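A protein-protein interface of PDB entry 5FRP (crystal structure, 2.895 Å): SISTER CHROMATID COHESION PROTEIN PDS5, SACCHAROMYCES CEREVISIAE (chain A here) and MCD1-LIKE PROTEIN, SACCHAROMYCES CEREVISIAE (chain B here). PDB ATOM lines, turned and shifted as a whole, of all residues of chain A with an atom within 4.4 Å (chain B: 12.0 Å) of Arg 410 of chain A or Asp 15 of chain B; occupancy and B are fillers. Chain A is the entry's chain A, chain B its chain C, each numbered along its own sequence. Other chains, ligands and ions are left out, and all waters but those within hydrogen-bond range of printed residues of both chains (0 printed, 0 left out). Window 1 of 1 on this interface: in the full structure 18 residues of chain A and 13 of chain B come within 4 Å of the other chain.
Of the 13 printed residues of chain B, 8 touch a printed residue of chain A. Printed residues of chain B that touch a printed residue of chain A: Leu 11, Met 12, Leu 13, Asp 15, Ala 16, Val 17, Thr 18 and Glu 19. Among the printed residues, Asp or Glu carboxylates within 4 Å of a Lys or Arg side-chain nitrogen of the other chain: Lys 502 of chain A with Asp 15 of chain B (3.4 Å).
The side-chain amino group of Lys 502 of chain A lies within salt-bridge range of the side-chain carboxylate of Asp 15 of chain B (3.4 Å). N of Glu 411 of chain A sits close to SD of Met 12 of chain B, at 3.6 Å. A ring nitrogen (NE2) of His 407 of chain A lies close to the side-chain sulfur of Met 12 of chain B, at 3.7 Å. O of Arg 410 of chain A lies within hydrogen-bond range of N of Leu 13 of chain B (2.7 Å). The backbone carbonyl oxygen (O) of Tyr 460 of chain A lies within hydrogen-bond range of the backbone NH (N) of Ala 16 of chain B (2.8 Å). The backbone NH (N) of Val 17 of chain B lies within hydrogen-bond range of the backbone carbonyl oxygen (O) of Tyr 460 of chain A (3.1 Å). O of Arg 410 of chain A lies close to SD of Met 12 of chain B, at 3.4 Å.
Arg 410 of chain A touches three residues of chain B. Of the printed residues of chain A, Asp 15 of chain B touches Arg 410, Tyr 460, Ile 461 and Lys 502. Of chain B, only Met 12 (3.3 Å) comes within 4 Å of His 407 of chain A. Ala 409 of chain A touches none of the printed residues of chain B. Of chain B, only Met 12 (3.4 Å) comes within 4 Å of Glu 411 of chain A. No residue of chain B comes within 4 Å of Asn 457 of chain A. Printed residues of chain A within 4 Å of Leu 11 of chain B: Lys 412. Printed residues of chain B within 4 Å of Lys 412 of chain A: Leu 11. Printed residues of chain B within 4 Å of Tyr 460 of chain A: Asp 15 (3.7 Å), Ala 16 (2.8 Å), Val 17 (3.1 Å), Thr 18 (3.8 Å) and Glu 19 (3.99 Å). Arg 20 of chain B touches none of the printed residues of chain A. Val 22 of chain B touches none of the printed residues of chain A. The nearest residue of chain B that does not touch Arg 410 of chain A is Glu 14 of chain B (4.4 Å).
The side-chain hydroxyl (OG1) of Thr 18 of chain B lies close to the backbone NH (N) of Glu 21 of chain B (3.2 Å). N of Arg 20 of chain B sits close to OG1 of Thr 18 of chain B (3.4 Å). The guanidinium group (NH2) of Arg 410 of chain A lies within hydrogen-bond range of the backbone carbonyl oxygen (O) of Asn 457 of chain A (3.3 Å). The side-chain hydroxyl (OH) of Tyr 460 of chain A is in hydrogen-bond range of the backbone carbonyl oxygen (O) of Lys 502 of chain A (2.7 Å).
Among the printed residues, merely in contact across the chains: Lys 412 of chain A with Leu 11 of chain B (3.3 Å), Lys 502 of chain A with Glu 19 of chain B (3.5 Å), Tyr 460 of chain A with Asp 15 of chain B (3.7 Å), Arg 410 of chain A with Asp 15 of chain B (3.7 Å), Tyr 460 of chain A with Thr 18 of chain B (3.8 Å), Ile 461 of chain A with Ala 16 of chain B (3.9 Å), Tyr 460 of chain A with Glu 19 of chain B (3.99 Å) and Ile 461 of chain A with Asp 15 of chain B (3.99 Å).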
ATOM      1  N   HIS A 407      12.641  27.669 -13.753  1.00  0.00           N
ATOM      2  CA  HIS A 407      11.807  26.489 -13.553  1.00  0.00           C
ATOM      3  C   HIS A 407      11.453  25.840 -14.883  1.00  0.00           C
ATOM      4  O   HIS A 407      11.469  24.614 -15.006  1.00  0.00           O
ATOM      5  CB  HIS A 407      10.531  26.862 -12.797  1.00  0.00           C
ATOM      6  CG  HIS A 407       9.522  25.758 -12.748  1.00  0.00           C
ATOM      7  ND1 HIS A 407       9.729  24.589 -12.047  1.00  0.00           N
ATOM      8  CD2 HIS A 407       8.299  25.647 -13.316  1.00  0.00           C
ATOM      9  CE1 HIS A 407       8.674  23.807 -12.185  1.00  0.00           C
ATOM     10  NE2 HIS A 407       7.792  24.424 -12.950  1.00  0.00           N
ATOM     11  N   LEU A 408      11.125  26.663 -15.874  1.00  0.00           N
ATOM     12  CA  LEU A 408      10.741  26.159 -17.191  1.00  0.00           C
ATOM     13  C   LEU A 408      11.872  25.382 -17.874  1.00  0.00           C
ATOM     14  O   LEU A 408      11.636  24.672 -18.851  1.00  0.00           O
ATOM     15  CB  LEU A 408      10.293  27.312 -18.093  1.00  0.00           C
ATOM     16  CG  LEU A 408       8.998  28.020 -17.683  1.00  0.00           C
ATOM     17  CD1 LEU A 408       8.730  29.190 -18.614  1.00  0.00           C
ATOM     18  CD2 LEU A 408       7.816  27.056 -17.672  1.00  0.00           C
ATOM     19  N   ALA A 409      13.091  25.512 -17.361  1.00  0.00           N
ATOM     20  CA  ALA A 409      14.244  24.825 -17.937  1.00  0.00           C
ATOM     21  C   ALA A 409      14.126  23.304 -17.818  1.00  0.00           C
ATOM     22  O   ALA A 409      14.823  22.567 -18.510  1.00  0.00           O
ATOM     23  CB  ALA A 409      15.519  25.302 -17.272  1.00  0.00           C
ATOM     24  N   ARG A 410      13.251  22.846 -16.929  1.00  0.00           N
ATOM     25  CA  ARG A 410      13.023  21.417 -16.729  1.00  0.00           C
ATOM     26  C   ARG A 410      11.666  21.002 -17.292  1.00  0.00           C
ATOM     27  O   ARG A 410      11.145  19.940 -16.950  1.00  0.00           O
ATOM     28  CB  ARG A 410      13.092  21.060 -15.242  1.00  0.00           C
ATOM     29  CG  ARG A 410      14.485  20.710 -14.747  1.00  0.00           C
ATOM     30  CD  ARG A 410      14.411  20.045 -13.377  1.00  0.00           C
ATOM     31  NE  ARG A 410      15.733  19.827 -12.791  1.00  0.00           N
ATOM     32  CZ  ARG A 410      16.452  18.713 -12.916  1.00  0.00           C
ATOM     33  NH1 ARG A 410      15.975  17.692 -13.618  1.00  0.00           N
ATOM     34  NH2 ARG A 410      17.643  18.610 -12.343  1.00  0.00           N
ATOM     35  N   GLU A 411      11.106  21.838 -18.160  1.00  0.00           N
ATOM     36  CA  GLU A 411       9.765  21.608 -18.683  1.00  0.00           C
ATOM     37  C   GLU A 411       9.756  20.556 -19.784  1.00  0.00           C
ATOM     38  O   GLU A 411      10.736  20.400 -20.514  1.00  0.00           O
ATOM     39  CB  GLU A 411       9.184  22.921 -19.210  1.00  0.00           C
ATOM     40  CG  GLU A 411       7.704  22.852 -19.535  1.00  0.00           C
ATOM     41  CD  GLU A 411       7.137  24.187 -19.979  1.00  0.00           C
ATOM     42  OE1 GLU A 411       7.867  24.969 -20.622  1.00  0.00           O
ATOM     43  OE2 GLU A 411       5.954  24.452 -19.676  1.00  0.00           O
ATOM     44  N   LYS A 412       8.642  19.837 -19.890  1.00  0.00           N
ATOM     45  CA  LYS A 412       8.458  18.849 -20.944  1.00  0.00           C
ATOM     46  C   LYS A 412       8.520  19.512 -22.312  1.00  0.00           C
ATOM     47  O   LYS A 412       9.241  19.052 -23.197  1.00  0.00           O
ATOM     48  CB  LYS A 412       7.120  18.124 -20.784  1.00  0.00           C
ATOM     49  CG  LYS A 412       7.047  17.161 -19.610  1.00  0.00           C
ATOM     50  CD  LYS A 412       7.723  15.834 -19.921  1.00  0.00           C
ATOM     51  CE  LYS A 412       7.622  14.860 -18.760  1.00  0.00           C
ATOM     52  NZ  LYS A 412       6.249  14.307 -18.595  1.00  0.00           N
ATOM     53  N   ASN A 457      22.693  20.589 -13.373  1.00  0.00           N
ATOM     54  CA  ASN A 457      21.755  19.555 -12.945  1.00  0.00           C
ATOM     55  C   ASN A 457      20.939  18.942 -14.088  1.00  0.00           C
ATOM     56  O   ASN A 457      20.391  17.851 -13.938  1.00  0.00           O
ATOM     57  CB  ASN A 457      20.809  20.114 -11.884  1.00  0.00           C
ATOM     58  CG  ASN A 457      21.434  20.101 -10.503  1.00  0.00           C
ATOM     59  OD1 ASN A 457      21.169  19.201  -9.707  1.00  0.00           O
ATOM     60  ND2 ASN A 457      22.269  21.092 -10.215  1.00  0.00           N
ATOM     61  N   TYR A 460      21.621  15.392 -15.379  1.00  0.00           N
ATOM     62  CA  TYR A 460      21.103  14.234 -14.661  1.00  0.00           C
ATOM     63  C   TYR A 460      19.838  13.658 -15.286  1.00  0.00           C
ATOM     64  O   TYR A 460      19.508  12.493 -15.061  1.00  0.00           O
ATOM     65  CB  TYR A 460      20.812  14.594 -13.202  1.00  0.00           C
ATOM     66  CG  TYR A 460      22.056  14.762 -12.362  1.00  0.00           C
ATOM     67  CD1 TYR A 460      22.666  13.664 -11.769  1.00  0.00           C
ATOM     68  CD2 TYR A 460      22.616  16.015 -12.157  1.00  0.00           C
ATOM     69  CE1 TYR A 460      23.801  13.811 -10.999  1.00  0.00           C
ATOM     70  CE2 TYR A 460      23.751  16.171 -11.387  1.00  0.00           C
ATOM     71  CZ  TYR A 460      24.338  15.065 -10.811  1.00  0.00           C
ATOM     72  OH  TYR A 460      25.469  15.215 -10.044  1.00  0.00           O
ATOM     73  N   ILE A 461      19.168  14.452 -16.100  1.00  0.00           N
ATOM     74  CA  ILE A 461      17.983  13.989 -16.773  1.00  0.00           C
ATOM     75  C   ILE A 461      18.395  13.030 -17.872  1.00  0.00           C
ATOM     76  O   ILE A 461      17.584  12.289 -18.385  1.00  0.00           O
ATOM     77  CB  ILE A 461      17.187  15.146 -17.362  1.00  0.00           C
ATOM     78  CG1 ILE A 461      17.913  15.747 -18.547  1.00  0.00           C
ATOM     79  CG2 ILE A 461      16.959  16.209 -16.325  1.00  0.00           C
ATOM     80  CD1 ILE A 461      17.290  15.326 -19.839  1.00  0.00           C
ATOM     81  N   LYS A 502      25.419  17.953  -6.158  1.00  0.00           N
ATOM     82  CA  LYS A 502      25.152  17.420  -7.488  1.00  0.00           C
ATOM     83  C   LYS A 502      25.932  18.196  -8.545  1.00  0.00           C
ATOM     84  O   LYS A 502      26.597  17.603  -9.395  1.00  0.00           O
ATOM     85  CB  LYS A 502      23.657  17.475  -7.805  1.00  0.00           C
ATOM     86  CG  LYS A 502      22.832  16.447  -7.050  1.00  0.00           C
ATOM     87  CD  LYS A 502      21.383  16.467  -7.514  1.00  0.00           C
ATOM     88  CE  LYS A 502      20.528  15.514  -6.696  1.00  0.00           C
ATOM     89  NZ  LYS A 502      19.087  15.643  -7.053  1.00  0.00           N
ATOM     90  N   LEU B  11       3.683  19.044 -17.260  1.00  0.00           N
ATOM     91  CA  LEU B  11       4.600  18.183 -16.521  1.00  0.00           C
ATOM     92  C   LEU B  11       6.016  18.745 -16.531  1.00  0.00           C
ATOM     93  O   LEU B  11       6.306  19.697 -17.258  1.00  0.00           O
ATOM     94  CB  LEU B  11       4.605  16.767 -17.099  1.00  0.00           C
ATOM     95  CG  LEU B  11       3.612  15.753 -16.529  1.00  0.00           C
ATOM     96  CD1 LEU B  11       3.945  15.434 -15.074  1.00  0.00           C
ATOM     97  CD2 LEU B  11       2.177  16.243 -16.656  1.00  0.00           C
ATOM     98  N   MET B  12       6.886  18.149 -15.722  1.00  0.00           N
ATOM     99  CA  MET B  12       8.284  18.554 -15.654  1.00  0.00           C
ATOM    100  C   MET B  12       9.199  17.339 -15.716  1.00  0.00           C
ATOM    101  O   MET B  12       8.889  16.294 -15.142  1.00  0.00           O
ATOM    102  CB  MET B  12       8.552  19.349 -14.374  1.00  0.00           C
ATOM    103  CG  MET B  12       7.926  20.737 -14.377  1.00  0.00           C
ATOM    104  SD  MET B  12       8.845  21.887 -15.417  1.00  0.00           S
ATOM    105  CE  MET B  12       7.525  22.970 -15.956  1.00  0.00           C
ATOM    106  N   LEU B  13      10.316  17.467 -16.404  1.00  0.00           N
ATOM    107  CA  LEU B  13      11.215  16.348 -16.513  1.00  0.00           C
ATOM    108  C   LEU B  13      11.726  15.992 -15.143  1.00  0.00           C
ATOM    109  O   LEU B  13      11.621  16.780 -14.221  1.00  0.00           O
ATOM    110  CB  LEU B  13      12.344  16.664 -17.462  1.00  0.00           C
ATOM    111  CG  LEU B  13      12.043  16.190 -18.874  1.00  0.00           C
ATOM    112  CD1 LEU B  13      12.864  16.958 -19.874  1.00  0.00           C
ATOM    113  CD2 LEU B  13      12.298  14.703 -19.012  1.00  0.00           C
ATOM    114  N   GLU B  14      12.267  14.790 -15.006  1.00  0.00           N
ATOM    115  CA  GLU B  14      12.786  14.333 -13.730  1.00  0.00           C
ATOM    116  C   GLU B  14      14.161  13.732 -13.900  1.00  0.00           C
ATOM    117  O   GLU B  14      14.383  12.932 -14.789  1.00  0.00           O
ATOM    118  CB  GLU B  14      11.848  13.302 -13.121  1.00  0.00           C
ATOM    119  CG  GLU B  14      11.623  12.083 -13.990  1.00  0.00           C
ATOM    120  CD  GLU B  14      10.953  10.956 -13.234  1.00  0.00           C
ATOM    121  OE1 GLU B  14       9.799  11.139 -12.805  1.00  0.00           O
ATOM    122  OE2 GLU B  14      11.582   9.895 -13.062  1.00  0.00           O
ATOM    123  N   ASP B  15      15.079  14.119 -13.030  1.00  0.00           N
ATOM    124  CA  ASP B  15      16.454  13.637 -13.099  1.00  0.00           C
ATOM    125  C   ASP B  15      16.489  12.116 -12.978  1.00  0.00           C
ATOM    126  O   ASP B  15      15.903  11.552 -12.054  1.00  0.00           O
ATOM    127  CB  ASP B  15      17.313  14.292 -12.014  1.00  0.00           C
ATOM    128  CG  ASP B  15      16.741  14.141 -10.619  1.00  0.00           C
ATOM    129  OD1 ASP B  15      15.512  13.969 -10.473  1.00  0.00           O
ATOM    130  OD2 ASP B  15      17.526  14.198  -9.648  1.00  0.00           O
ATOM    131  N   ALA B  16      17.078  11.485 -13.988  1.00  0.00           N
ATOM    132  CA  ALA B  16      17.079  10.042 -14.111  1.00  0.00           C
ATOM    133  C   ALA B  16      18.403   9.301 -14.062  1.00  0.00           C
ATOM    134  O   ALA B  16      18.528   8.235 -14.640  1.00  0.00           O
ATOM    135  CB  ALA B  16      16.365   9.674 -15.392  1.00  0.00           C
ATOM    136  N   VAL B  17      19.383   9.846 -13.369  1.00  0.00           N
ATOM    137  CA  VAL B  17      20.660   9.170 -13.176  1.00  0.00           C
ATOM    138  C   VAL B  17      21.158   9.461 -11.768  1.00  0.00           C
ATOM    139  O   VAL B  17      20.753  10.448 -11.154  1.00  0.00           O
ATOM    140  CB  VAL B  17      21.730   9.597 -14.214  1.00  0.00           C
ATOM    141  CG1 VAL B  17      21.160   9.542 -15.623  1.00  0.00           C
ATOM    142  CG2 VAL B  17      22.283  10.983 -13.910  1.00  0.00           C
ATOM    143  N   THR B  18      22.036   8.605 -11.261  1.00  0.00           N
ATOM    144  CA  THR B  18      22.584   8.786  -9.925  1.00  0.00           C
ATOM    145  C   THR B  18      23.791   9.716  -9.961  1.00  0.00           C
ATOM    146  O   THR B  18      24.287  10.052 -11.036  1.00  0.00           O
ATOM    147  CB  THR B  18      23.007   7.445  -9.298  1.00  0.00           C
ATOM    148  OG1 THR B  18      24.078   6.878 -10.064  1.00  0.00           O
ATOM    149  CG2 THR B  18      21.844   6.467  -9.264  1.00  0.00           C
ATOM    150  N   GLU B  19      24.259  10.130  -8.787  1.00  0.00           N
ATOM    151  CA  GLU B  19      25.437  10.983  -8.705  1.00  0.00           C
ATOM    152  C   GLU B  19      26.671  10.194  -9.119  1.00  0.00           C
ATOM    153  O   GLU B  19      27.658  10.767  -9.583  1.00  0.00           O
ATOM    154  CB  GLU B  19      25.613  11.533  -7.290  1.00  0.00           C
ATOM    155  CG  GLU B  19      24.506  12.486  -6.877  1.00  0.00           C
ATOM    156  CD  GLU B  19      24.747  13.131  -5.527  1.00  0.00           C
ATOM    157  OE1 GLU B  19      25.866  13.004  -4.985  1.00  0.00           O
ATOM    158  OE2 GLU B  19      23.808  13.769  -5.006  1.00  0.00           O
ATOM    159  N   ARG B  20      26.604   8.878  -8.943  1.00  0.00           N
ATOM    160  CA  ARG B  20      27.706   7.992  -9.288  1.00  0.00           C
ATOM    161  C   ARG B  20      27.889   7.945 -10.799  1.00  0.00           C
ATOM    162  O   ARG B  20      28.939   8.328 -11.315  1.00  0.00           O
ATOM    163  CB  ARG B  20      27.443   6.583  -8.761  1.00  0.00           C
ATOM    164  CG  ARG B  20      27.273   6.530  -7.255  1.00  0.00           C
ATOM    165  CD  ARG B  20      27.150   5.097  -6.769  1.00  0.00           C
ATOM    166  NE  ARG B  20      26.891   5.052  -5.333  1.00  0.00           N
ATOM    167  CZ  ARG B  20      26.750   3.933  -4.629  1.00  0.00           C
ATOM    168  NH1 ARG B  20      26.840   2.749  -5.223  1.00  0.00           N
ATOM    169  NH2 ARG B  20      26.515   4.003  -3.327  1.00  0.00           N
ATOM    170  N   GLU B  21      26.857   7.474 -11.491  1.00  0.00           N
ATOM    171  CA  GLU B  21      26.888   7.357 -12.943  1.00  0.00           C
ATOM    172  C   GLU B  21      26.217   8.561 -13.599  1.00  0.00           C
ATOM    173  O   GLU B  21      24.993   8.604 -13.729  1.00  0.00           O
ATOM    174  CB  GLU B  21      26.230   6.052 -13.405  1.00  0.00           C
ATOM    175  CG  GLU B  21      24.882   5.751 -12.768  1.00  0.00           C
ATOM    176  CD  GLU B  21      24.202   4.538 -13.372  1.00  0.00           C
ATOM    177  OE1 GLU B  21      24.779   3.943 -14.307  1.00  0.00           O
ATOM    178  OE2 GLU B  21      23.098   4.175 -12.916  1.00  0.00           O
ATOM    179  N   VAL B  22      27.027   9.531 -14.006  1.00  0.00           N
ATOM    180  CA  VAL B  22      26.542  10.717 -14.695  1.00  0.00           C
ATOM    181  C   VAL B  22      27.579  11.084 -15.748  1.00  0.00           C
ATOM    182  O   VAL B  22      28.745  11.302 -15.428  1.00  0.00           O
ATOM    183  CB  VAL B  22      26.273  11.882 -13.712  1.00  0.00           C
ATOM    184  CG1 VAL B  22      27.481  12.156 -12.825  1.00  0.00           C
ATOM    185  CG2 VAL B  22      25.852  13.141 -14.462  1.00  0.00           C
ATOM    186  N   LEU B  23      27.151  11.130 -17.007  1.00  0.00           N
ATOM    187  CA  LEU B  23      28.070  11.311 -18.127  1.00  0.00           C
ATOM    188  C   LEU B  23      29.040  10.139 -18.223  1.00  0.00           C
ATOM    189  O   LEU B  23      30.178  10.304 -18.656  1.00  0.00           O
ATOM    190  CB  LEU B  23      28.848  12.623 -17.991  1.00  0.00           C
ATOM    191  CG  LEU B  23      28.012  13.887 -17.771  1.00  0.00           C
ATOM    192  CD1 LEU B  23      28.925  15.094 -17.645  1.00  0.00           C
ATOM    193  CD2 LEU B  23      27.010  14.083 -18.899  1.00  0.00           C
